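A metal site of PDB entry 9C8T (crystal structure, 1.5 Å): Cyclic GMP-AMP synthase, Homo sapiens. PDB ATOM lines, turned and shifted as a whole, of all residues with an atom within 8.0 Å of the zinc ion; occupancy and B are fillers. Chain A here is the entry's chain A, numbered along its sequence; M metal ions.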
ATOM      1  N   LEU A 232       8.495   1.839 -20.143  1.00  0.00           N
ATOM      2  CA  LEU A 232       7.419   2.064 -19.172  1.00  0.00           C
ATOM      3  C   LEU A 232       7.355   0.949 -18.155  1.00  0.00           C
ATOM      4  O   LEU A 232       7.042   1.214 -16.988  1.00  0.00           O
ATOM      5  CB  LEU A 232       6.060   2.208 -19.868  1.00  0.00           C
ATOM      6  CG  LEU A 232       5.934   3.623 -20.400  1.00  0.00           C
ATOM      7  CD1 LEU A 232       4.820   3.692 -21.419  1.00  0.00           C
ATOM      8  CD2 LEU A 232       5.557   4.558 -19.210  1.00  0.00           C
ATOM      9  N   ASN A 234       9.936  -0.705 -17.010  1.00  0.00           N
ATOM     10  CA  ASN A 234      11.206  -0.789 -16.307  1.00  0.00           C
ATOM     11  C   ASN A 234      11.727   0.652 -16.279  1.00  0.00           C
ATOM     12  O   ASN A 234      12.659   1.021 -16.967  1.00  0.00           O
ATOM     13  CB  ASN A 234      12.164  -1.749 -17.009  1.00  0.00           C
ATOM     14  CG  ASN A 234      13.309  -2.126 -16.139  1.00  0.00           C
ATOM     15  OD1 ASN A 234      13.449  -1.688 -14.991  1.00  0.00           O
ATOM     16  ND2 ASN A 234      14.151  -3.000 -16.661  1.00  0.00           N
ATOM     17  N   HIS A 235      11.059   1.480 -15.481  1.00  0.00           N
ATOM     18  CA  HIS A 235      11.039   2.923 -15.704  1.00  0.00           C
ATOM     19  C   HIS A 235      11.809   3.723 -14.697  1.00  0.00           C
ATOM     20  O   HIS A 235      11.811   4.947 -14.793  1.00  0.00           O
ATOM     21  CB  HIS A 235       9.575   3.445 -15.684  1.00  0.00           C
ATOM     22  CG  HIS A 235       8.885   3.182 -14.408  1.00  0.00           C
ATOM     23  ND1 HIS A 235       7.809   2.330 -14.301  1.00  0.00           N
ATOM     24  CD2 HIS A 235       9.183   3.577 -13.140  1.00  0.00           C
ATOM     25  CE1 HIS A 235       7.453   2.233 -13.030  1.00  0.00           C
ATOM     26  NE2 HIS A 235       8.255   2.998 -12.305  1.00  0.00           N
ATOM     27  N   GLY A 236      12.408   3.083 -13.707  1.00  0.00           N
ATOM     28  CA  GLY A 236      13.042   3.870 -12.670  1.00  0.00           C
ATOM     29  C   GLY A 236      14.540   3.936 -12.836  1.00  0.00           C
ATOM     30  O   GLY A 236      15.143   3.149 -13.560  1.00  0.00           O
ATOM     31  N   LYS A 237      15.164   4.885 -12.164  1.00  0.00           N
ATOM     32  CA  LYS A 237      16.615   4.812 -12.047  1.00  0.00           C
ATOM     33  C   LYS A 237      17.020   3.622 -11.168  1.00  0.00           C
ATOM     34  O   LYS A 237      17.948   2.860 -11.499  1.00  0.00           O
ATOM     35  CB  LYS A 237      17.130   6.092 -11.434  1.00  0.00           C
ATOM     36  CG  LYS A 237      18.661   5.997 -11.289  1.00  0.00           C
ATOM     37  CD  LYS A 237      19.324   7.343 -10.904  1.00  0.00           C
ATOM     38  CE  LYS A 237      19.255   8.293 -12.079  1.00  0.00           C
ATOM     39  NZ  LYS A 237      19.936   7.655 -13.265  1.00  0.00           N
ATOM     40  N   SER A 238      16.315   3.407 -10.071  1.00  0.00           N
ATOM     41  CA  SER A 238      16.474   2.190  -9.289  1.00  0.00           C
ATOM     42  C   SER A 238      15.887   0.994 -10.019  1.00  0.00           C
ATOM     43  O   SER A 238      14.736   1.015 -10.481  1.00  0.00           O
ATOM     44  CB  SER A 238      15.750   2.342  -7.976  1.00  0.00           C
ATOM     45  OG  SER A 238      15.824   1.085  -7.312  1.00  0.00           O
ATOM     46  N   THR A 240      14.799  -1.497  -8.585  1.00  0.00           N
ATOM     47  CA  THR A 240      13.647  -1.927  -7.799  1.00  0.00           C
ATOM     48  C   THR A 240      12.520  -0.904  -7.711  1.00  0.00           C
ATOM     49  O   THR A 240      11.594  -1.113  -6.908  1.00  0.00           O
ATOM     50  CB  THR A 240      14.107  -2.443  -6.413  1.00  0.00           C
ATOM     51  OG1 THR A 240      14.996  -1.476  -5.792  1.00  0.00           O
ATOM     52  CG2 THR A 240      14.849  -3.741  -6.596  1.00  0.00           C
ATOM     53  N   CYS A 241      12.519   0.108  -8.590  1.00  0.00           N
ATOM     54  CA  CYS A 241      11.421   1.078  -8.628  1.00  0.00           C
ATOM     55  C   CYS A 241      10.105   0.351  -8.756  1.00  0.00           C
ATOM     56  O   CYS A 241       9.955  -0.526  -9.596  1.00  0.00           O
ATOM     57  CB  CYS A 241      11.660   2.070  -9.759  1.00  0.00           C
ATOM     58  SG  CYS A 241      10.550   3.565  -9.580  1.00  0.00           S
ATOM     59  N   CYS A 242       9.169   0.706  -7.884  1.00  0.00           N
ATOM     60  CA  CYS A 242       7.818   0.108  -7.922  1.00  0.00           C
ATOM     61  C   CYS A 242       7.783  -1.378  -7.571  1.00  0.00           C
ATOM     62  O   CYS A 242       6.747  -2.016  -7.783  1.00  0.00           O
ATOM     63  CB  CYS A 242       7.003   0.393  -9.182  1.00  0.00           C
ATOM     64  SG  CYS A 242       6.697   2.219  -9.305  1.00  0.00           S
ATOM     65  N   GLU A 243       8.864  -1.956  -7.026  1.00  0.00           N
ATOM     66  CA  GLU A 243       8.848  -3.355  -6.605  1.00  0.00           C
ATOM     67  C   GLU A 243       8.669  -3.513  -5.111  1.00  0.00           C
ATOM     68  O   GLU A 243       8.617  -4.640  -4.602  1.00  0.00           O
ATOM     69  CB  GLU A 243      10.147  -4.070  -7.004  1.00  0.00           C
ATOM     70  CG  GLU A 243      10.186  -4.405  -8.475  1.00  0.00           C
ATOM     71  CD  GLU A 243      11.226  -5.467  -8.825  1.00  0.00           C
ATOM     72  OE1 GLU A 243      12.020  -5.864  -7.926  1.00  0.00           O
ATOM     73  OE2 GLU A 243      11.219  -5.923  -9.990  1.00  0.00           O
ATOM     74  N   ASN A 244       8.627  -2.419  -4.376  1.00  0.00           N
ATOM     75  CA  ASN A 244       8.404  -2.482  -2.945  1.00  0.00           C
ATOM     76  C   ASN A 244       7.722  -1.197  -2.521  1.00  0.00           C
ATOM     77  O   ASN A 244       7.706  -0.204  -3.255  1.00  0.00           O
ATOM     78  CB  ASN A 244       9.695  -2.688  -2.157  1.00  0.00           C
ATOM     79  CG  ASN A 244      10.694  -1.574  -2.385  1.00  0.00           C
ATOM     80  OD1 ASN A 244      10.535  -0.471  -1.859  1.00  0.00           O
ATOM     81  ND2 ASN A 244      11.774  -1.861  -3.124  1.00  0.00           N
ATOM     82  N   GLU A 247       9.455   2.263  -2.745  1.00  0.00           N
ATOM     83  CA  GLU A 247       9.866   2.807  -4.034  1.00  0.00           C
ATOM     84  C   GLU A 247       8.687   2.877  -5.013  1.00  0.00           C
ATOM     85  O   GLU A 247       8.836   2.633  -6.228  1.00  0.00           O
ATOM     86  CB  GLU A 247      11.016   1.994  -4.618  1.00  0.00           C
ATOM     87  CG  GLU A 247      12.310   1.956  -3.786  1.00  0.00           C
ATOM     88  CD  GLU A 247      13.431   1.243  -4.528  1.00  0.00           C
ATOM     89  OE1 GLU A 247      13.951   1.769  -5.535  1.00  0.00           O
ATOM     90  OE2 GLU A 247      13.761   0.127  -4.119  1.00  0.00           O
ATOM     91  N   LYS A 248       7.488   3.279  -4.531  1.00  0.00           N
ATOM     92  CA  LYS A 248       6.298   3.355  -5.384  1.00  0.00           C
ATOM     93  C   LYS A 248       6.226   4.748  -5.978  1.00  0.00           C
ATOM     94  O   LYS A 248       5.600   5.659  -5.418  1.00  0.00           O
ATOM     95  CB  LYS A 248       5.040   3.018  -4.593  1.00  0.00           C
ATOM     96  CG  LYS A 248       4.955   1.551  -4.217  1.00  0.00           C
ATOM     97  CD  LYS A 248       4.666   0.664  -5.431  1.00  0.00           C
ATOM     98  CE  LYS A 248       4.616  -0.828  -5.049  1.00  0.00           C
ATOM     99  NZ  LYS A 248       4.187  -1.637  -6.232  1.00  0.00           N
ATOM    100  N   CYS A 249       6.873   4.941  -7.131  1.00  0.00           N
ATOM    101  CA  CYS A 249       6.948   6.258  -7.707  1.00  0.00           C
ATOM    102  C   CYS A 249       5.616   6.609  -8.366  1.00  0.00           C
ATOM    103  O   CYS A 249       4.729   5.776  -8.528  1.00  0.00           O
ATOM    104  CB  CYS A 249       8.128   6.349  -8.695  1.00  0.00           C
ATOM    105  SG  CYS A 249       7.768   5.629 -10.392  1.00  0.00           S
ATOM    106  N   CYS A 250       5.516   7.860  -8.817  1.00  0.00           N
ATOM    107  CA  CYS A 250       4.277   8.338  -9.416  1.00  0.00           C
ATOM    108  C   CYS A 250       4.357   8.521 -10.926  1.00  0.00           C
ATOM    109  O   CYS A 250       3.498   9.166 -11.496  1.00  0.00           O
ATOM    110  CB  CYS A 250       3.775   9.555  -8.633  1.00  0.00           C
ATOM    111  SG  CYS A 250       4.647  11.086  -8.951  1.00  0.00           S
ATOM    112  N   ARG A 251       5.351   7.940 -11.577  1.00  0.00           N
ATOM    113  CA  ARG A 251       5.493   8.137 -13.010  1.00  0.00           C
ATOM    114  C   ARG A 251       4.262   7.647 -13.801  1.00  0.00           C
ATOM    115  O   ARG A 251       3.706   8.408 -14.607  1.00  0.00           O
ATOM    116  CB  ARG A 251       6.735   7.406 -13.522  1.00  0.00           C
ATOM    117  CG  ARG A 251       8.050   8.146 -13.198  1.00  0.00           C
ATOM    118  CD  ARG A 251       9.213   7.411 -13.885  1.00  0.00           C
ATOM    119  NE  ARG A 251      10.524   7.997 -13.538  1.00  0.00           N
ATOM    120  CZ  ARG A 251      11.271   7.572 -12.511  1.00  0.00           C
ATOM    121  NH1 ARG A 251      10.815   6.662 -11.644  1.00  0.00           N
ATOM    122  NH2 ARG A 251      12.529   8.036 -12.411  1.00  0.00           N
ATOM    123  N   LYS A 252       3.822   6.398 -13.588  1.00  0.00           N
ATOM    124  CA  LYS A 252       2.670   5.887 -14.352  1.00  0.00           C
ATOM    125  C   LYS A 252       1.390   6.638 -13.996  1.00  0.00           C
ATOM    126  O   LYS A 252       0.583   6.911 -14.898  1.00  0.00           O
ATOM    127  CB  LYS A 252       2.502   4.366 -14.161  1.00  0.00           C
ATOM    128  CG  LYS A 252       3.562   3.594 -14.891  1.00  0.00           C
ATOM    129  CD  LYS A 252       3.195   2.093 -15.031  1.00  0.00           C
ATOM    130  CE  LYS A 252       4.281   1.465 -15.854  1.00  0.00           C
ATOM    131  NZ  LYS A 252       4.070  -0.026 -16.099  1.00  0.00           N
ATOM    132  N   ASP A 297      14.443   9.009  -9.200  1.00  0.00           N
ATOM    133  CA  ASP A 297      13.195   8.513  -8.627  1.00  0.00           C
ATOM    134  C   ASP A 297      12.634   9.453  -7.564  1.00  0.00           C
ATOM    135  O   ASP A 297      11.421   9.505  -7.364  1.00  0.00           O
ATOM    136  CB  ASP A 297      13.409   7.104  -8.053  1.00  0.00           C
ATOM    137  CG  ASP A 297      13.784   6.084  -9.134  1.00  0.00           C
ATOM    138  OD1 ASP A 297      13.503   6.345 -10.344  1.00  0.00           O
ATOM    139  OD2 ASP A 297      14.375   5.040  -8.756  1.00  0.00           O
ATOM    140  N   TRP A 300       9.878  11.816  -8.454  1.00  0.00           N
ATOM    141  CA  TRP A 300       8.581  11.197  -8.749  1.00  0.00           C
ATOM    142  C   TRP A 300       8.061  10.514  -7.497  1.00  0.00           C
ATOM    143  O   TRP A 300       7.488   9.426  -7.528  1.00  0.00           O
ATOM    144  CB  TRP A 300       8.736  10.208  -9.898  1.00  0.00           C
ATOM    145  CG  TRP A 300       9.201  10.848 -11.151  1.00  0.00           C
ATOM    146  CD1 TRP A 300      10.496  10.943 -11.603  1.00  0.00           C
ATOM    147  CD2 TRP A 300       8.383  11.466 -12.127  1.00  0.00           C
ATOM    148  NE1 TRP A 300      10.507  11.597 -12.799  1.00  0.00           N
ATOM    149  CE2 TRP A 300       9.225  11.928 -13.159  1.00  0.00           C
ATOM    150  CE3 TRP A 300       6.988  11.659 -12.228  1.00  0.00           C
ATOM    151  CZ2 TRP A 300       8.741  12.528 -14.302  1.00  0.00           C
ATOM    152  CZ3 TRP A 300       6.481  12.297 -13.350  1.00  0.00           C
ATOM    153  CH2 TRP A 300       7.377  12.751 -14.378  1.00  0.00           C
HETATM  154 ZN    ZN M   1       8.397   3.342 -10.266  1.00  0.00          ZN
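A ring nitrogen (ND1) of His 235 is in hydrogen-bond range of the backbone carbonyl oxygen of Leu 232 (3.0 Å).
N of Cys 242 is in hydrogen-bond range of O of Glu 247.
NZ of Lys 248 lies within hydrogen-bond range of O of Cys 242 (3.0 Å).
The guanidinium group (NH1) of Arg 251 sits close to the side-chain sulfur (SG) of Cys 241.
The side-chain sulfur of Cys 249 lies close to the guanidinium group of Arg 251 (3.5 Å).
Of the 19 residues printed, 4 come within 4 Å of the zinc ion.
The zinc ion is bound by NE2 of His 235 (2.1 Å), SG of Cys 242 (2.3 Å), SG of Cys 241 (2.3 Å) and SG of Cys 249 (2.4 Å).
The zinc ion has four donor atoms within binding distance.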
